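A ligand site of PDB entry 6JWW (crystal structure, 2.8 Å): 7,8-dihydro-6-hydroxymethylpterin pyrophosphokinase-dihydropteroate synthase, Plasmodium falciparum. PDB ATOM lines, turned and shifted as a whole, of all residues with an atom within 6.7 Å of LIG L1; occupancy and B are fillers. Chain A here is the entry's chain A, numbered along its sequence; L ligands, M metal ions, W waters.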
ATOM      1  N   ASN A  21       0.563  10.139 -13.991  1.00  0.00           N
ATOM      2  CA  ASN A  21       0.121  11.088 -14.999  1.00  0.00           C
ATOM      3  C   ASN A  21       1.346  11.537 -15.796  1.00  0.00           C
ATOM      4  O   ASN A  21       2.409  11.782 -15.215  1.00  0.00           O
ATOM      5  CB  ASN A  21      -0.600  12.272 -14.333  1.00  0.00           C
ATOM      6  CG  ASN A  21      -1.206  13.236 -15.330  1.00  0.00           C
ATOM      7  OD1 ASN A  21      -2.121  12.882 -16.095  1.00  0.00           O
ATOM      8  ND2 ASN A  21      -0.697  14.470 -15.338  1.00  0.00           N
ATOM      9  N   LEU A  22       1.211  11.594 -17.118  1.00  0.00           N
ATOM     10  CA  LEU A  22       2.298  12.041 -18.001  1.00  0.00           C
ATOM     11  C   LEU A  22       1.843  13.238 -18.787  1.00  0.00           C
ATOM     12  O   LEU A  22       0.758  13.234 -19.370  1.00  0.00           O
ATOM     13  CB  LEU A  22       2.754  10.921 -18.964  1.00  0.00           C
ATOM     14  CG  LEU A  22       3.479   9.645 -18.487  1.00  0.00           C
ATOM     15  CD1 LEU A  22       4.033   8.898 -19.677  1.00  0.00           C
ATOM     16  CD2 LEU A  22       4.599   9.897 -17.493  1.00  0.00           C
ATOM     17  N   GLY A  23       2.674  14.272 -18.800  1.00  0.00           N
ATOM     18  CA  GLY A  23       2.303  15.525 -19.431  1.00  0.00           C
ATOM     19  C   GLY A  23       3.446  16.153 -20.186  1.00  0.00           C
ATOM     20  O   GLY A  23       4.586  16.121 -19.728  1.00  0.00           O
ATOM     21  N   THR A  24       3.109  16.707 -21.345  1.00  0.00           N
ATOM     22  CA  THR A  24       3.990  17.553 -22.146  1.00  0.00           C
ATOM     23  C   THR A  24       3.145  18.595 -22.875  1.00  0.00           C
ATOM     24  O   THR A  24       1.934  18.447 -22.980  1.00  0.00           O
ATOM     25  CB  THR A  24       4.834  16.718 -23.159  1.00  0.00           C
ATOM     26  OG1 THR A  24       5.791  17.578 -23.793  1.00  0.00           O
ATOM     27  CG2 THR A  24       3.963  16.050 -24.235  1.00  0.00           C
ATOM     28  N   THR A  57      -5.239  18.488 -24.567  1.00  0.00           N
ATOM     29  CA  THR A  57      -6.031  18.934 -23.444  1.00  0.00           C
ATOM     30  C   THR A  57      -5.844  20.412 -23.074  1.00  0.00           C
ATOM     31  O   THR A  57      -4.732  20.956 -23.113  1.00  0.00           O
ATOM     32  CB  THR A  57      -5.837  17.938 -22.269  1.00  0.00           C
ATOM     33  OG1 THR A  57      -6.917  18.056 -21.345  1.00  0.00           O
ATOM     34  CG2 THR A  57      -4.535  18.133 -21.595  1.00  0.00           C
ATOM     35  N   VAL A  58      -6.970  21.052 -22.748  1.00  0.00           N
ATOM     36  CA  VAL A  58      -6.985  22.460 -22.354  1.00  0.00           C
ATOM     37  C   VAL A  58      -6.321  22.642 -20.977  1.00  0.00           C
ATOM     38  O   VAL A  58      -6.629  21.876 -20.040  1.00  0.00           O
ATOM     39  CB  VAL A  58      -8.432  23.044 -22.427  1.00  0.00           C
ATOM     40  CG1 VAL A  58      -8.651  24.192 -21.445  1.00  0.00           C
ATOM     41  CG2 VAL A  58      -8.714  23.483 -23.848  1.00  0.00           C
ATOM     42  N   PRO A  59      -5.387  23.629 -20.882  1.00  0.00           N
ATOM     43  CA  PRO A  59      -4.631  23.908 -19.661  1.00  0.00           C
ATOM     44  C   PRO A  59      -5.542  24.257 -18.517  1.00  0.00           C
ATOM     45  O   PRO A  59      -6.533  24.995 -18.693  1.00  0.00           O
ATOM     46  CB  PRO A  59      -3.774  25.127 -20.037  1.00  0.00           C
ATOM     47  CG  PRO A  59      -3.619  25.034 -21.507  1.00  0.00           C
ATOM     48  CD  PRO A  59      -4.961  24.535 -21.968  1.00  0.00           C
ATOM     49  N   GLU A  60      -5.192  23.706 -17.362  1.00  0.00           N
ATOM     50  CA  GLU A  60      -5.996  23.788 -16.172  1.00  0.00           C
ATOM     51  C   GLU A  60      -5.136  24.366 -15.058  1.00  0.00           C
ATOM     52  O   GLU A  60      -4.960  23.721 -14.007  1.00  0.00           O
ATOM     53  CB  GLU A  60      -6.409  22.392 -15.780  1.00  0.00           C
ATOM     54  CG  GLU A  60      -7.796  22.274 -15.217  1.00  0.00           C
ATOM     55  CD  GLU A  60      -8.715  21.536 -16.164  1.00  0.00           C
ATOM     56  OE1 GLU A  60      -9.939  21.522 -15.902  1.00  0.00           O
ATOM     57  OE2 GLU A  60      -8.211  20.963 -17.164  1.00  0.00           O
ATOM     58  N   TYR A  61      -4.571  25.555 -15.267  1.00  0.00           N
ATOM     59  CA  TYR A  61      -3.761  26.184 -14.226  1.00  0.00           C
ATOM     60  C   TYR A  61      -4.628  26.674 -13.053  1.00  0.00           C
ATOM     61  O   TYR A  61      -4.105  27.167 -12.054  1.00  0.00           O
ATOM     62  CB  TYR A  61      -2.939  27.357 -14.779  1.00  0.00           C
ATOM     63  CG  TYR A  61      -1.754  26.978 -15.627  1.00  0.00           C
ATOM     64  CD1 TYR A  61      -0.661  26.271 -15.084  1.00  0.00           C
ATOM     65  CD2 TYR A  61      -1.688  27.353 -16.978  1.00  0.00           C
ATOM     66  CE1 TYR A  61       0.438  25.947 -15.867  1.00  0.00           C
ATOM     67  CE2 TYR A  61      -0.601  27.034 -17.767  1.00  0.00           C
ATOM     68  CZ  TYR A  61       0.459  26.318 -17.217  1.00  0.00           C
ATOM     69  OH  TYR A  61       1.548  25.981 -17.992  1.00  0.00           O
ATOM     70  N   ILE A  62      -5.946  26.482 -13.193  1.00  0.00           N
ATOM     71  CA  ILE A  62      -6.951  27.001 -12.277  1.00  0.00           C
ATOM     72  C   ILE A  62      -7.590  25.877 -11.432  1.00  0.00           C
ATOM     73  O   ILE A  62      -8.692  26.022 -10.875  1.00  0.00           O
ATOM     74  CB  ILE A  62      -7.985  27.854 -13.084  1.00  0.00           C
ATOM     75  CG1 ILE A  62      -8.554  29.009 -12.222  1.00  0.00           C
ATOM     76  CG2 ILE A  62      -9.044  27.010 -13.808  1.00  0.00           C
ATOM     77  CD1 ILE A  62      -7.642  30.229 -12.118  1.00  0.00           C
ATOM     78  N   TYR A 162      -1.863  23.747 -25.649  1.00  0.00           N
ATOM     79  CA  TYR A 162      -2.510  22.568 -25.091  1.00  0.00           C
ATOM     80  C   TYR A 162      -1.500  21.672 -24.378  1.00  0.00           C
ATOM     81  O   TYR A 162      -0.309  21.748 -24.651  1.00  0.00           O
ATOM     82  CB  TYR A 162      -3.143  21.739 -26.205  1.00  0.00           C
ATOM     83  CG  TYR A 162      -4.347  22.352 -26.889  1.00  0.00           C
ATOM     84  CD1 TYR A 162      -5.628  22.235 -26.331  1.00  0.00           C
ATOM     85  CD2 TYR A 162      -4.210  23.009 -28.116  1.00  0.00           C
ATOM     86  CE1 TYR A 162      -6.735  22.771 -26.972  1.00  0.00           C
ATOM     87  CE2 TYR A 162      -5.313  23.545 -28.766  1.00  0.00           C
ATOM     88  CZ  TYR A 162      -6.561  23.420 -28.192  1.00  0.00           C
ATOM     89  OH  TYR A 162      -7.646  23.971 -28.847  1.00  0.00           O
ATOM     90  N   PHE A 163      -1.994  20.814 -23.484  1.00  0.00           N
ATOM     91  CA  PHE A 163      -1.182  19.739 -22.922  1.00  0.00           C
ATOM     92  C   PHE A 163      -1.438  18.415 -23.618  1.00  0.00           C
ATOM     93  O   PHE A 163      -2.548  18.141 -24.084  1.00  0.00           O
ATOM     94  CB  PHE A 163      -1.436  19.579 -21.427  1.00  0.00           C
ATOM     95  CG  PHE A 163      -0.815  20.639 -20.576  1.00  0.00           C
ATOM     96  CD1 PHE A 163      -1.445  21.877 -20.405  1.00  0.00           C
ATOM     97  CD2 PHE A 163       0.388  20.408 -19.923  1.00  0.00           C
ATOM     98  CE1 PHE A 163      -0.872  22.863 -19.613  1.00  0.00           C
ATOM     99  CE2 PHE A 163       0.966  21.367 -19.115  1.00  0.00           C
ATOM    100  CZ  PHE A 163       0.342  22.611 -18.965  1.00  0.00           C
ATOM    101  N   TYR A 164      -0.401  17.601 -23.667  1.00  0.00           N
ATOM    102  CA  TYR A 164      -0.477  16.235 -24.164  1.00  0.00           C
ATOM    103  C   TYR A 164      -0.275  15.268 -23.011  1.00  0.00           C
ATOM    104  O   TYR A 164       0.819  15.176 -22.435  1.00  0.00           O
ATOM    105  CB  TYR A 164       0.461  16.042 -25.368  1.00  0.00           C
ATOM    106  CG  TYR A 164       0.018  17.010 -26.423  1.00  0.00           C
ATOM    107  CD1 TYR A 164      -1.034  16.694 -27.290  1.00  0.00           C
ATOM    108  CD2 TYR A 164       0.576  18.299 -26.491  1.00  0.00           C
ATOM    109  CE1 TYR A 164      -1.485  17.616 -28.221  1.00  0.00           C
ATOM    110  CE2 TYR A 164       0.129  19.226 -27.410  1.00  0.00           C
ATOM    111  CZ  TYR A 164      -0.906  18.885 -28.266  1.00  0.00           C
ATOM    112  OH  TYR A 164      -1.363  19.795 -29.199  1.00  0.00           O
ATOM    113  N   ASN A 165      -1.371  14.598 -22.684  1.00  0.00           N
ATOM    114  CA  ASN A 165      -1.546  13.870 -21.434  1.00  0.00           C
ATOM    115  C   ASN A 165      -1.769  12.372 -21.586  1.00  0.00           C
ATOM    116  O   ASN A 165      -2.350  11.918 -22.572  1.00  0.00           O
ATOM    117  CB  ASN A 165      -2.718  14.481 -20.661  1.00  0.00           C
ATOM    118  CG  ASN A 165      -2.310  15.682 -19.836  1.00  0.00           C
ATOM    119  OD1 ASN A 165      -3.054  16.667 -19.747  1.00  0.00           O
ATOM    120  ND2 ASN A 165      -1.142  15.607 -19.205  1.00  0.00           N
ATOM    121  N   ASP A 208       6.320  16.251 -17.592  1.00  0.00           N
ATOM    122  CA  ASP A 208       5.870  16.230 -16.192  1.00  0.00           C
ATOM    123  C   ASP A 208       5.226  14.897 -15.815  1.00  0.00           C
ATOM    124  O   ASP A 208       4.248  14.495 -16.438  1.00  0.00           O
ATOM    125  CB  ASP A 208       4.899  17.382 -15.927  1.00  0.00           C
ATOM    126  CG  ASP A 208       4.568  17.545 -14.469  1.00  0.00           C
ATOM    127  OD1 ASP A 208       5.499  17.521 -13.633  1.00  0.00           O
ATOM    128  OD2 ASP A 208       3.380  17.685 -14.118  1.00  0.00           O
ATOM    129  N   ASP A 210       3.525  12.804 -12.666  1.00  0.00           N
ATOM    130  CA  ASP A 210       2.893  12.900 -11.342  1.00  0.00           C
ATOM    131  C   ASP A 210       2.428  11.533 -10.856  1.00  0.00           C
ATOM    132  O   ASP A 210       1.993  10.706 -11.667  1.00  0.00           O
ATOM    133  CB  ASP A 210       1.675  13.833 -11.402  1.00  0.00           C
ATOM    134  CG  ASP A 210       2.024  15.215 -11.932  1.00  0.00           C
ATOM    135  OD1 ASP A 210       3.063  15.788 -11.521  1.00  0.00           O
ATOM    136  OD2 ASP A 210       1.234  15.755 -12.748  1.00  0.00           O
ATOM    137  N   ARG A 326      -8.711  18.313 -11.820  1.00  0.00           N
ATOM    138  CA  ARG A 326      -8.351  18.519 -13.227  1.00  0.00           C
ATOM    139  C   ARG A 326      -9.091  17.549 -14.165  1.00  0.00           C
ATOM    140  O   ARG A 326      -9.092  16.339 -13.945  1.00  0.00           O
ATOM    141  CB  ARG A 326      -6.843  18.436 -13.424  1.00  0.00           C
ATOM    142  CG  ARG A 326      -6.099  19.692 -13.014  1.00  0.00           C
ATOM    143  CD  ARG A 326      -4.830  19.869 -13.827  1.00  0.00           C
ATOM    144  NE  ARG A 326      -4.015  20.950 -13.265  1.00  0.00           N
ATOM    145  CZ  ARG A 326      -2.924  20.758 -12.525  1.00  0.00           C
ATOM    146  NH1 ARG A 326      -2.479  19.544 -12.252  1.00  0.00           N
ATOM    147  NH2 ARG A 326      -2.258  21.811 -12.052  1.00  0.00           N
ATOM    148  N   SER A 328      -8.432  16.806 -17.392  1.00  0.00           N
ATOM    149  CA  SER A 328      -7.459  16.013 -18.115  1.00  0.00           C
ATOM    150  C   SER A 328      -7.028  14.779 -17.315  1.00  0.00           C
ATOM    151  O   SER A 328      -6.614  13.766 -17.899  1.00  0.00           O
ATOM    152  CB  SER A 328      -6.223  16.855 -18.451  1.00  0.00           C
ATOM    153  OG  SER A 328      -5.576  17.286 -17.265  1.00  0.00           O
ATOM    154  N   ILE A 329      -7.130  14.871 -15.998  1.00  0.00           N
ATOM    155  CA  ILE A 329      -6.817  13.731 -15.151  1.00  0.00           C
ATOM    156  C   ILE A 329      -7.960  12.701 -15.151  1.00  0.00           C
ATOM    157  O   ILE A 329      -7.704  11.525 -15.413  1.00  0.00           O
ATOM    158  CB  ILE A 329      -6.344  14.122 -13.731  1.00  0.00           C
ATOM    159  CG1 ILE A 329      -5.138  15.080 -13.838  1.00  0.00           C
ATOM    160  CG2 ILE A 329      -6.056  12.870 -12.907  1.00  0.00           C
ATOM    161  CD1 ILE A 329      -4.446  15.457 -12.536  1.00  0.00           C
ATOM    162  N   ASN A 372     -10.937  18.926 -25.376  1.00  0.00           N
ATOM    163  CA  ASN A 372     -10.057  17.895 -24.854  1.00  0.00           C
ATOM    164  C   ASN A 372     -10.207  16.614 -25.682  1.00  0.00           C
ATOM    165  O   ASN A 372     -11.129  15.832 -25.462  1.00  0.00           O
ATOM    166  CB  ASN A 372     -10.265  17.676 -23.353  1.00  0.00           C
ATOM    167  CG  ASN A 372     -10.106  18.963 -22.553  1.00  0.00           C
ATOM    168  OD1 ASN A 372      -9.031  19.263 -22.029  1.00  0.00           O
ATOM    169  ND2 ASN A 372     -11.173  19.741 -22.481  1.00  0.00           N
HETATM  170  N1  LIG L   1      -0.225  20.525 -15.576  1.00  0.00           N
HETATM  171  C1  LIG L   1      -0.070  21.571 -14.741  1.00  0.00           C
HETATM  172  C2  LIG L   1      -1.030  22.726 -14.727  1.00  0.00           C
HETATM  173  N2  LIG L   1      -2.158  22.564 -15.657  1.00  0.00           N
HETATM  174  N3  LIG L   1      -3.308  21.382 -17.318  1.00  0.00           N
HETATM  175  C3  LIG L   1      -3.420  20.292 -18.127  1.00  0.00           C
HETATM  176  N4  LIG L   1      -4.469  20.226 -18.953  1.00  0.00           N
HETATM  177  N5  LIG L   1      -2.518  19.271 -18.139  1.00  0.00           N
HETATM  178  C4  LIG L   1      -1.456  19.271 -17.333  1.00  0.00           C
HETATM  179  O1  LIG L   1      -0.636  18.317 -17.357  1.00  0.00           O
HETATM  180  C5  LIG L   1      -1.268  20.435 -16.419  1.00  0.00           C
HETATM  181  C6  LIG L   1      -2.274  21.506 -16.461  1.00  0.00           C
HETATM  182  C7  LIG L   1       1.145  21.591 -13.844  1.00  0.00           C
HETATM  183  O2  LIG L   1       2.317  21.232 -14.600  1.00  0.00           O
HETATM  184  P1  LG2 L   2       1.660  19.486 -10.038  1.00  0.00           P
HETATM  185  O1  LG2 L   2       0.607  20.497 -10.462  1.00  0.00           O
HETATM  186  O2  LG2 L   2       1.935  18.394 -11.044  1.00  0.00           O
HETATM  187  O3  LG2 L   2       1.550  19.000  -8.606  1.00  0.00           O
HETATM  188  P2  LG2 L   2       3.668  21.115 -11.186  1.00  0.00           P
HETATM  189  O4  LG2 L   2       3.680  20.200 -12.389  1.00  0.00           O
HETATM  190  O5  LG2 L   2       2.993  22.474 -11.283  1.00  0.00           O
HETATM  191  O6  LG2 L   2       3.012  20.348  -9.945  1.00  0.00           O
HETATM  192  P3  LG2 L   2       6.203  20.180 -10.312  1.00  0.00           P
HETATM  193  O7  LG2 L   2       7.518  20.822  -9.935  1.00  0.00           O
HETATM  194  O8  LG2 L   2       6.202  19.104 -11.371  1.00  0.00           O
HETATM  195  O9  LG2 L   2       5.195  21.371 -10.723  1.00  0.00           O
HETATM  196  O10 LG2 L   2       5.510  19.575  -8.984  1.00  0.00           O
HETATM  197  C1  LG2 L   2       5.303  20.393  -7.828  1.00  0.00           C
HETATM  198  C2  LG2 L   2       5.759  19.686  -6.574  1.00  0.00           C
HETATM  199  O11 LG2 L   2       4.666  19.032  -5.937  1.00  0.00           O
HETATM  200  C3  LG2 L   2       6.756  18.557  -6.785  1.00  0.00           C
HETATM  201  O12 LG2 L   2       8.080  19.066  -6.932  1.00  0.00           O
HETATM  202  C4  LG2 L   2       6.625  17.710  -5.545  1.00  0.00           C
HETATM  203  O13 LG2 L   2       7.533  18.160  -4.527  1.00  0.00           O
HETATM  204  C5  LG2 L   2       5.197  18.006  -5.090  1.00  0.00           C
HETATM  205  N1  LG2 L   2       4.335  16.803  -5.106  1.00  0.00           N
HETATM  206  C6  LG2 L   2       3.518  16.443  -4.096  1.00  0.00           C
HETATM  207  N2  LG2 L   2       2.845  15.299  -4.374  1.00  0.00           N
HETATM  208  C7  LG2 L   2       3.220  14.918  -5.599  1.00  0.00           C
HETATM  209  C8  LG2 L   2       2.889  13.793  -6.518  1.00  0.00           C
HETATM  210  N3  LG2 L   2       1.995  12.854  -6.145  1.00  0.00           N
HETATM  211  N4  LG2 L   2       3.509  13.760  -7.711  1.00  0.00           N
HETATM  212  C9  LG2 L   2       4.394  14.690  -8.109  1.00  0.00           C
HETATM  213  N5  LG2 L   2       4.739  15.729  -7.329  1.00  0.00           N
HETATM  214  C10 LG2 L   2       4.204  15.899  -6.089  1.00  0.00           C
HETATM  215 MG    MG M   1       3.831  17.705 -11.682  1.00  0.00          MG
HETATM  216  O   HOH W   1       5.165  21.264 -14.939  1.00  0.00           O
HETATM  217  O   HOH W   2       1.367  18.415 -15.890  1.00  0.00           O
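The backbone NH of Val 58 is in hydrogen-bond range of the side-chain amide oxygen of Asn 372 (2.8 Å).
The side-chain hydroxyl of Thr 57 lies within hydrogen-bond range of the side-chain amide oxygen of Asn 372 (2.5 Å).
O of Glu 60 is in hydrogen-bond range of NE of Arg 326, at 3.0 Å.
The backbone carbonyl oxygen (O) of Phe 163 is in hydrogen-bond range of the backbone NH (N) of Thr 57, 2.8 Å away.
ND2 of Asn 165 sits at hydrogen-bond distance from O of Leu 22.
The backbone NH (N) of Asp 208 is in hydrogen-bond range of the backbone carbonyl oxygen (O) of Gly 23 (2.8 Å).
O4 of LG2 L2 sits close to O2 of LIG L1, at 2.8 Å.
NE of Arg 326 lies close to N2 of LIG L1 (3.4 Å).
Thr 57 touches LIG L1 (CG2 to N4, 3.4 Å).
CA of Pro 59 touches N3 of LIG L1, at 3.7 Å.
Tyr 61 touches LIG L1 (CD1 to C2, 3.6 Å).
CG of Phe 163 touches N5 of LIG L1, 3.3 Å away.
Asp 208 touches LIG L1.
OG of Ser 328 touches N4 of LIG L1, 3.6 Å away.
Ten residues have an atom within 4 Å of LIG L1: Thr 57, Val 58, Pro 59, Glu 60, Tyr 61, Phe 163, Asn 165, Asp 208, Arg 326 and Ser 328.
Along chain A the residues within 4 Å of LIG L1 span positions 57 to 328.
A nitrogen (N4) of LIG L1 is in hydrogen-bond range of the backbone carbonyl oxygen (O) of Val 58, at 2.9 Å.
The guanidinium group (NH2) of Arg 326 is in salt-bridge range of an oxygen (O1) of LG2 L2.
The side-chain amide oxygen (OD1) of Asn 165 sits at hydrogen-bond distance from a nitrogen (N5) of LIG L1 (3.1 Å).
N3 of LIG L1 sits at hydrogen-bond distance from N of Glu 60 (3.0 Å).
O of Glu 60 lies within hydrogen-bond range of N2 of LIG L1 (3.5 Å).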
